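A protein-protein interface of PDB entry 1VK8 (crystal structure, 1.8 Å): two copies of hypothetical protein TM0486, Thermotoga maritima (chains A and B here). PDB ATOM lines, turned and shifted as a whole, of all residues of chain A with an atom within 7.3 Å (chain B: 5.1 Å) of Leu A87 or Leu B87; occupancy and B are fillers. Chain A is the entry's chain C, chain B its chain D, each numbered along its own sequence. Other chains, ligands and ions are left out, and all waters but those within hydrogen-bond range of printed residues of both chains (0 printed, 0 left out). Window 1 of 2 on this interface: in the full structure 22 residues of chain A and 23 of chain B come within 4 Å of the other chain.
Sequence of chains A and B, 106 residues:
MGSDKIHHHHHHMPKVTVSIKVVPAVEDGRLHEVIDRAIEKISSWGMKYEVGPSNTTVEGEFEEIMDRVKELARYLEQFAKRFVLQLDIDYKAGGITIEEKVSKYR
N of Asp A88 lies within hydrogen-bond range of O of Ser A19 (2.9 Å). The backbone NH of Gln A86 lies within hydrogen-bond range of the backbone carbonyl oxygen of Lys A21 (2.9 Å). The backbone carbonyl oxygen of Asp B88 lies within hydrogen-bond range of the backbone NH of Ser B19 (2.9 Å).
CG1 of Val A84 touches OD1 of Asp B88, 3.4 Å away. O of Ile B89 touches CA of Val A84, 3.3 Å away. Leu B87 touches Leu A85 (O to O, 3.8 Å). Asp B88 touches Leu A85 (C to O, 3.8 Å). Leu B87 touches Gln A86. Leu B85 touches Leu A87. Gln B86 touches Leu A87. O of Leu B85 touches C of Asp A88 (3.7 Å).
O of Leu A85 is in hydrogen-bond range of N of Ile B89. The side-chain amide nitrogen of Gln A86 sits at hydrogen-bond distance from the side-chain carboxylate of Asp B88 (3.2 Å). The backbone NH of Leu B87 sits at hydrogen-bond distance from the backbone carbonyl oxygen of Leu A87, at 2.9 Å. The side-chain carboxylate (OD1) of Asp A88 lies within hydrogen-bond range of the side-chain amide nitrogen (NE2) of Gln B86 (3.3 Å). O of Leu B85 lies within hydrogen-bond range of N of Ile A89.
Leu A85 touches Leu B87, and with the chains exchanged Leu A87 touches Leu B85. Leu A85 touches Ile B89, and with the chains exchanged Ile A89 touches Leu B85. Gln A86 touches Asp B88, and with the chains exchanged Asp A88 touches Gln B86. Leu A87 touches its own counterpart, Leu B87. Positions printed for both chains: 18, 19, 20, 66, 69, 85, 86, 87, 88 and 89. Of the 13 pairs that touch across the chains among the printed residues, 11 have their exchanged pair printed and touching as well.
Of the printed residues of chain B, Leu A87 touches Leu B85 (3.8 Å), Gln B86 (3.1 Å) and Leu B87 (2.9 Å). Leu B87 touches just these residues of chain A: Leu A85, Gln A86 and Leu A87. Printed residues of chain A within 4 Å of Ile B89: Val A84 (3.3 Å) and Leu A85 (2.8 Å). Of the printed residues of chain B, Leu A85 touches Leu B87, Asp B88 and Ile B89. Val B69 touches none of the printed residues of chain A. Ser A19 touches none of the printed residues of chain B. The nearest residue of chain B that does not touch Leu A87 is Ile B89 (4.7 Å). The nearest residue of chain A that does not touch Leu B87 is Ile A89 (4.7 Å). The nearest printed residue of chain B that does not touch Asp A88 is Leu B87 (5.1 Å).
Hydrophobic or aromatic side chains of chain A within 4 Å of the printed part of chain B: Val A84, Leu A85, Leu A87 and Ile A89. Of the 10 printed residues of chain B, 5 touch a printed residue of chain A. Along chain B the printed residues that touch a printed residue of chain A span positions 85 to 89. Among the printed residues, 13 pairs touch across the chains. Among the printed residues, no Asp or Glu carboxylate lies within 4 Å of a Lys or Arg side-chain nitrogen of the other chain.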
ATOM      1  N   VAL A  18      -8.075  30.305  18.741  1.00  0.00           N
ATOM      2  CA  VAL A  18      -7.681  29.920  20.085  1.00  0.00           C
ATOM      3  C   VAL A  18      -8.839  29.160  20.695  1.00  0.00           C
ATOM      4  O   VAL A  18      -9.938  29.706  20.880  1.00  0.00           O
ATOM      5  CB  VAL A  18      -7.365  31.158  20.969  1.00  0.00           C
ATOM      6  CG1 VAL A  18      -6.910  30.743  22.350  1.00  0.00           C
ATOM      7  CG2 VAL A  18      -6.274  32.033  20.269  1.00  0.00           C
ATOM      8  N   SER A  19      -8.598  27.891  20.996  1.00  0.00           N
ATOM      9  CA  SER A  19      -9.567  27.070  21.676  1.00  0.00           C
ATOM     10  C   SER A  19      -9.241  27.065  23.141  1.00  0.00           C
ATOM     11  O   SER A  19      -8.095  26.892  23.532  1.00  0.00           O
ATOM     12  CB  SER A  19      -9.551  25.667  21.066  1.00  0.00           C
ATOM     13  OG  SER A  19      -9.848  25.780  19.680  1.00  0.00           O
ATOM     14  N   ILE A  20     -10.266  27.289  23.951  1.00  0.00           N
ATOM     15  CA  ILE A  20     -10.141  27.534  25.366  1.00  0.00           C
ATOM     16  C   ILE A  20     -10.926  26.444  26.082  1.00  0.00           C
ATOM     17  O   ILE A  20     -12.098  26.187  25.759  1.00  0.00           O
ATOM     18  CB  ILE A  20     -10.734  28.911  25.711  1.00  0.00           C
ATOM     19  CG1 ILE A  20     -10.000  30.016  24.975  1.00  0.00           C
ATOM     20  CG2 ILE A  20     -10.720  29.164  27.222  1.00  0.00           C
ATOM     21  CD1 ILE A  20     -10.688  31.339  25.053  1.00  0.00           C
ATOM     22  N   LYS A  21     -10.285  25.823  27.068  1.00  0.00           N
ATOM     23  CA  LYS A  21     -10.918  24.812  27.906  1.00  0.00           C
ATOM     24  C   LYS A  21     -10.698  25.177  29.358  1.00  0.00           C
ATOM     25  O   LYS A  21      -9.580  25.460  29.776  1.00  0.00           O
ATOM     26  CB  LYS A  21     -10.346  23.422  27.632  1.00  0.00           C
ATOM     27  CG  LYS A  21     -10.992  22.298  28.389  1.00  0.00           C
ATOM     28  CD  LYS A  21     -10.287  20.973  28.182  1.00  0.00           C
ATOM     29  CE  LYS A  21     -11.104  19.807  28.681  1.00  0.00           C
ATOM     30  NZ  LYS A  21     -12.102  19.343  27.649  1.00  0.00           N
ATOM     31  N   TRP A  45     -16.936  39.060  24.202  1.00  0.00           N
ATOM     32  CA  TRP A  45     -15.745  39.641  23.596  1.00  0.00           C
ATOM     33  C   TRP A  45     -16.009  40.207  22.227  1.00  0.00           C
ATOM     34  O   TRP A  45     -15.150  40.913  21.716  1.00  0.00           O
ATOM     35  CB  TRP A  45     -14.604  38.621  23.472  1.00  0.00           C
ATOM     36  CG  TRP A  45     -14.098  38.065  24.791  1.00  0.00           C
ATOM     37  CD1 TRP A  45     -14.406  38.492  26.042  1.00  0.00           C
ATOM     38  CD2 TRP A  45     -13.182  36.980  24.945  1.00  0.00           C
ATOM     39  NE1 TRP A  45     -13.751  37.720  26.970  1.00  0.00           N
ATOM     40  CE2 TRP A  45     -13.001  36.777  26.321  1.00  0.00           C
ATOM     41  CE3 TRP A  45     -12.495  36.144  24.043  1.00  0.00           C
ATOM     42  CZ2 TRP A  45     -12.160  35.781  26.820  1.00  0.00           C
ATOM     43  CZ3 TRP A  45     -11.663  35.156  24.539  1.00  0.00           C
ATOM     44  CH2 TRP A  45     -11.503  34.993  25.915  1.00  0.00           C
ATOM     45  N   PHE A  62      -4.481  37.997  17.919  1.00  0.00           N
ATOM     46  CA  PHE A  62      -3.778  37.225  18.959  1.00  0.00           C
ATOM     47  C   PHE A  62      -3.574  37.956  20.299  1.00  0.00           C
ATOM     48  O   PHE A  62      -3.921  37.446  21.350  1.00  0.00           O
ATOM     49  CB  PHE A  62      -2.440  36.752  18.389  1.00  0.00           C
ATOM     50  CG  PHE A  62      -1.597  36.013  19.364  1.00  0.00           C
ATOM     51  CD1 PHE A  62      -2.023  34.849  19.926  1.00  0.00           C
ATOM     52  CD2 PHE A  62      -0.359  36.496  19.711  1.00  0.00           C
ATOM     53  CE1 PHE A  62      -1.241  34.197  20.856  1.00  0.00           C
ATOM     54  CE2 PHE A  62       0.404  35.840  20.614  1.00  0.00           C
ATOM     55  CZ  PHE A  62      -0.040  34.701  21.188  1.00  0.00           C
ATOM     56  N   ILE A  65      -6.821  38.585  22.184  1.00  0.00           N
ATOM     57  CA  ILE A  65      -7.309  37.346  22.822  1.00  0.00           C
ATOM     58  C   ILE A  65      -6.494  37.061  24.102  1.00  0.00           C
ATOM     59  O   ILE A  65      -7.058  36.744  25.148  1.00  0.00           O
ATOM     60  CB  ILE A  65      -7.287  36.135  21.837  1.00  0.00           C
ATOM     61  CG1 ILE A  65      -8.287  36.286  20.703  1.00  0.00           C
ATOM     62  CG2 ILE A  65      -7.621  34.826  22.575  1.00  0.00           C
ATOM     63  CD1 ILE A  65      -7.937  35.355  19.477  1.00  0.00           C
ATOM     64  N   MET A  66      -5.175  37.212  24.040  1.00  0.00           N
ATOM     65  CA  MET A  66      -4.336  36.971  25.232  1.00  0.00           C
ATOM     66  C   MET A  66      -4.757  37.898  26.377  1.00  0.00           C
ATOM     67  O   MET A  66      -4.886  37.474  27.504  1.00  0.00           O
ATOM     68  CB  MET A  66      -2.849  37.128  24.909  1.00  0.00           C
ATOM     69  CG  MET A  66      -2.308  36.116  23.947  1.00  0.00           C
ATOM     70  SD  MET A  66      -2.686  34.225  24.522  1.00  0.00           S
ATOM     71  CE  MET A  66      -4.112  33.780  23.289  1.00  0.00           C
ATOM     72  N   VAL A  69      -7.973  36.676  27.783  1.00  0.00           N
ATOM     73  CA  VAL A  69      -7.728  35.499  28.600  1.00  0.00           C
ATOM     74  C   VAL A  69      -7.293  35.930  30.004  1.00  0.00           C
ATOM     75  O   VAL A  69      -7.710  35.326  30.968  1.00  0.00           O
ATOM     76  CB  VAL A  69      -6.724  34.533  27.925  1.00  0.00           C
ATOM     77  CG1 VAL A  69      -6.255  33.480  28.892  1.00  0.00           C
ATOM     78  CG2 VAL A  69      -7.356  33.909  26.686  1.00  0.00           C
ATOM     79  N   LEU A  72     -10.490  36.782  31.665  1.00  0.00           N
ATOM     80  CA  LEU A  72     -11.237  35.551  31.882  1.00  0.00           C
ATOM     81  C   LEU A  72     -10.805  34.826  33.161  1.00  0.00           C
ATOM     82  O   LEU A  72     -11.648  34.444  33.981  1.00  0.00           O
ATOM     83  CB  LEU A  72     -11.104  34.605  30.683  1.00  0.00           C
ATOM     84  CG  LEU A  72     -11.832  33.248  30.812  1.00  0.00           C
ATOM     85  CD1 LEU A  72     -13.310  33.463  30.947  1.00  0.00           C
ATOM     86  CD2 LEU A  72     -11.519  32.391  29.631  1.00  0.00           C
ATOM     87  N   VAL A  84      -7.953  24.416  35.932  1.00  0.00           N
ATOM     88  CA  VAL A  84      -7.068  24.325  34.804  1.00  0.00           C
ATOM     89  C   VAL A  84      -7.680  25.145  33.671  1.00  0.00           C
ATOM     90  O   VAL A  84      -8.882  25.067  33.398  1.00  0.00           O
ATOM     91  CB  VAL A  84      -6.882  22.857  34.348  1.00  0.00           C
ATOM     92  CG1 VAL A  84      -6.149  22.779  33.008  1.00  0.00           C
ATOM     93  CG2 VAL A  84      -6.184  22.048  35.429  1.00  0.00           C
ATOM     94  N   LEU A  85      -6.846  25.941  33.028  1.00  0.00           N
ATOM     95  CA  LEU A  85      -7.220  26.719  31.870  1.00  0.00           C
ATOM     96  C   LEU A  85      -6.234  26.393  30.741  1.00  0.00           C
ATOM     97  O   LEU A  85      -5.023  26.595  30.871  1.00  0.00           O
ATOM     98  CB  LEU A  85      -7.182  28.194  32.218  1.00  0.00           C
ATOM     99  CG  LEU A  85      -7.424  29.188  31.084  1.00  0.00           C
ATOM    100  CD1 LEU A  85      -8.822  29.094  30.503  1.00  0.00           C
ATOM    101  CD2 LEU A  85      -7.135  30.607  31.570  1.00  0.00           C
ATOM    102  N   GLN A  86      -6.757  25.876  29.642  1.00  0.00           N
ATOM    103  CA  GLN A  86      -5.949  25.427  28.524  1.00  0.00           C
ATOM    104  C   GLN A  86      -6.292  26.207  27.284  1.00  0.00           C
ATOM    105  O   GLN A  86      -7.474  26.421  26.980  1.00  0.00           O
ATOM    106  CB  GLN A  86      -6.117  23.928  28.286  1.00  0.00           C
ATOM    107  CG  GLN A  86      -5.603  23.097  29.447  1.00  0.00           C
ATOM    108  CD  GLN A  86      -5.811  21.617  29.269  1.00  0.00           C
ATOM    109  OE1 GLN A  86      -6.680  21.214  28.514  1.00  0.00           O
ATOM    110  NE2 GLN A  86      -5.047  20.811  29.988  1.00  0.00           N
ATOM    111  N   LEU A  87      -5.254  26.694  26.609  1.00  0.00           N
ATOM    112  CA  LEU A  87      -5.367  27.379  25.324  1.00  0.00           C
ATOM    113  C   LEU A  87      -4.630  26.579  24.252  1.00  0.00           C
ATOM    114  O   LEU A  87      -3.477  26.158  24.445  1.00  0.00           O
ATOM    115  CB  LEU A  87      -4.723  28.750  25.390  1.00  0.00           C
ATOM    116  CG  LEU A  87      -5.113  29.735  26.488  1.00  0.00           C
ATOM    117  CD1 LEU A  87      -4.476  31.075  26.151  1.00  0.00           C
ATOM    118  CD2 LEU A  87      -6.585  29.879  26.644  1.00  0.00           C
ATOM    119  N   ASP A  88      -5.286  26.393  23.109  1.00  0.00           N
ATOM    120  CA  ASP A  88      -4.688  25.731  21.952  1.00  0.00           C
ATOM    121  C   ASP A  88      -4.776  26.737  20.807  1.00  0.00           C
ATOM    122  O   ASP A  88      -5.840  26.978  20.218  1.00  0.00           O
ATOM    123  CB  ASP A  88      -5.445  24.407  21.714  1.00  0.00           C
ATOM    124  CG  ASP A  88      -5.117  23.732  20.395  1.00  0.00           C
ATOM    125  OD1 ASP A  88      -3.995  23.909  19.930  1.00  0.00           O
ATOM    126  OD2 ASP A  88      -5.914  22.951  19.788  1.00  0.00           O
ATOM    127  N   ILE A  89      -3.640  27.360  20.513  1.00  0.00           N
ATOM    128  CA  ILE A  89      -3.566  28.474  19.558  1.00  0.00           C
ATOM    129  C   ILE A  89      -3.043  27.963  18.224  1.00  0.00           C
ATOM    130  O   ILE A  89      -2.004  27.338  18.188  1.00  0.00           O
ATOM    131  CB  ILE A  89      -2.621  29.570  20.084  1.00  0.00           C
ATOM    132  CG1 ILE A  89      -3.082  30.082  21.456  1.00  0.00           C
ATOM    133  CG2 ILE A  89      -2.488  30.725  19.054  1.00  0.00           C
ATOM    134  CD1 ILE A  89      -1.962  30.521  22.292  1.00  0.00           C
ATOM    135  N   VAL B  18       2.436  27.481  34.105  1.00  0.00           N
ATOM    136  CA  VAL B  18       1.975  27.436  32.727  1.00  0.00           C
ATOM    137  C   VAL B  18       2.913  26.520  31.988  1.00  0.00           C
ATOM    138  O   VAL B  18       4.121  26.781  31.929  1.00  0.00           O
ATOM    139  CB  VAL B  18       1.968  28.849  32.102  1.00  0.00           C
ATOM    140  CG1 VAL B  18       1.482  28.864  30.616  1.00  0.00           C
ATOM    141  CG2 VAL B  18       1.062  29.755  32.937  1.00  0.00           C
ATOM    142  N   SER B  19       2.377  25.431  31.459  1.00  0.00           N
ATOM    143  CA  SER B  19       3.157  24.533  30.613  1.00  0.00           C
ATOM    144  C   SER B  19       2.938  24.911  29.159  1.00  0.00           C
ATOM    145  O   SER B  19       1.799  25.054  28.719  1.00  0.00           O
ATOM    146  CB  SER B  19       2.743  23.098  30.894  1.00  0.00           C
ATOM    147  OG  SER B  19       2.970  22.853  32.265  1.00  0.00           O
ATOM    148  N   ILE B  20       4.031  25.068  28.418  1.00  0.00           N
ATOM    149  CA  ILE B  20       4.004  25.570  27.061  1.00  0.00           C
ATOM    150  C   ILE B  20       4.522  24.525  26.117  1.00  0.00           C
ATOM    151  O   ILE B  20       5.596  23.990  26.339  1.00  0.00           O
ATOM    152  CB  ILE B  20       4.904  26.826  26.973  1.00  0.00           C
ATOM    153  CG1 ILE B  20       4.459  27.868  27.997  1.00  0.00           C
ATOM    154  CG2 ILE B  20       4.926  27.404  25.542  1.00  0.00           C
ATOM    155  CD1 ILE B  20       5.412  29.088  28.048  1.00  0.00           C
ATOM    156  N   MET B  66       1.362  35.748  30.399  1.00  0.00           N
ATOM    157  CA  MET B  66       0.533  35.974  29.211  1.00  0.00           C
ATOM    158  C   MET B  66       1.204  37.012  28.285  1.00  0.00           C
ATOM    159  O   MET B  66       1.227  36.815  27.074  1.00  0.00           O
ATOM    160  CB  MET B  66      -0.878  36.409  29.589  1.00  0.00           C
ATOM    161  CG  MET B  66      -1.708  35.384  30.313  1.00  0.00           C
ATOM    162  SD  MET B  66      -1.717  33.601  29.396  1.00  0.00           S
ATOM    163  CE  MET B  66      -0.420  32.671  30.435  1.00  0.00           C
ATOM    164  N   VAL B  69       4.061  35.355  26.547  1.00  0.00           N
ATOM    165  CA  VAL B  69       3.574  34.459  25.502  1.00  0.00           C
ATOM    166  C   VAL B  69       3.303  35.222  24.222  1.00  0.00           C
ATOM    167  O   VAL B  69       3.597  34.702  23.161  1.00  0.00           O
ATOM    168  CB  VAL B  69       2.359  33.636  25.968  1.00  0.00           C
ATOM    169  CG1 VAL B  69       1.650  32.990  24.820  1.00  0.00           C
ATOM    170  CG2 VAL B  69       2.799  32.607  27.002  1.00  0.00           C
ATOM    171  N   LEU B  85       0.511  26.491  19.320  1.00  0.00           N
ATOM    172  CA  LEU B  85       1.014  26.891  20.611  1.00  0.00           C
ATOM    173  C   LEU B  85      -0.029  26.576  21.687  1.00  0.00           C
ATOM    174  O   LEU B  85      -1.140  27.050  21.617  1.00  0.00           O
ATOM    175  CB  LEU B  85       1.353  28.354  20.591  1.00  0.00           C
ATOM    176  CG  LEU B  85       1.810  29.012  21.899  1.00  0.00           C
ATOM    177  CD1 LEU B  85       3.032  28.415  22.438  1.00  0.00           C
ATOM    178  CD2 LEU B  85       2.012  30.485  21.671  1.00  0.00           C
ATOM    179  N   GLN B  86       0.349  25.778  22.671  1.00  0.00           N
ATOM    180  CA  GLN B  86      -0.574  25.300  23.681  1.00  0.00           C
ATOM    181  C   GLN B  86      -0.088  25.710  25.057  1.00  0.00           C
ATOM    182  O   GLN B  86       1.092  25.601  25.343  1.00  0.00           O
ATOM    183  CB  GLN B  86      -0.739  23.778  23.579  1.00  0.00           C
ATOM    184  CG  GLN B  86      -1.327  23.325  22.263  1.00  0.00           C
ATOM    185  CD  GLN B  86      -1.534  21.844  22.188  1.00  0.00           C
ATOM    186  OE1 GLN B  86      -0.762  21.089  22.747  1.00  0.00           O
ATOM    187  NE2 GLN B  86      -2.532  21.426  21.451  1.00  0.00           N
ATOM    188  N   LEU B  87      -0.993  26.279  25.843  1.00  0.00           N
ATOM    189  CA  LEU B  87      -0.738  26.652  27.242  1.00  0.00           C
ATOM    190  C   LEU B  87      -1.652  25.827  28.107  1.00  0.00           C
ATOM    191  O   LEU B  87      -2.865  25.770  27.865  1.00  0.00           O
ATOM    192  CB  LEU B  87      -1.031  28.136  27.462  1.00  0.00           C
ATOM    193  CG  LEU B  87      -0.396  29.136  26.511  1.00  0.00           C
ATOM    194  CD1 LEU B  87      -0.745  30.526  27.034  1.00  0.00           C
ATOM    195  CD2 LEU B  87       1.102  28.981  26.394  1.00  0.00           C
ATOM    196  N   ASP B  88      -1.080  25.200  29.125  1.00  0.00           N
ATOM    197  CA  ASP B  88      -1.832  24.484  30.136  1.00  0.00           C
ATOM    198  C   ASP B  88      -1.512  25.213  31.462  1.00  0.00           C
ATOM    199  O   ASP B  88      -0.405  25.120  32.001  1.00  0.00           O
ATOM    200  CB  ASP B  88      -1.377  23.041  30.090  1.00  0.00           C
ATOM    201  CG  ASP B  88      -1.950  22.189  31.177  1.00  0.00           C
ATOM    202  OD1 ASP B  88      -3.017  22.543  31.707  1.00  0.00           O
ATOM    203  OD2 ASP B  88      -1.423  21.101  31.522  1.00  0.00           O
ATOM    204  N   ILE B  89      -2.492  25.959  31.954  1.00  0.00           N
ATOM    205  CA  ILE B  89      -2.321  26.858  33.086  1.00  0.00           C
ATOM    206  C   ILE B  89      -2.982  26.227  34.297  1.00  0.00           C
ATOM    207  O   ILE B  89      -4.140  25.804  34.223  1.00  0.00           O
ATOM    208  CB  ILE B  89      -2.975  28.234  32.794  1.00  0.00           C
ATOM    209  CG1 ILE B  89      -2.379  28.851  31.527  1.00  0.00           C
ATOM    210  CG2 ILE B  89      -2.866  29.178  34.025  1.00  0.00           C
ATOM    211  CD1 ILE B  89      -3.304  29.781  30.824  1.00  0.00           C
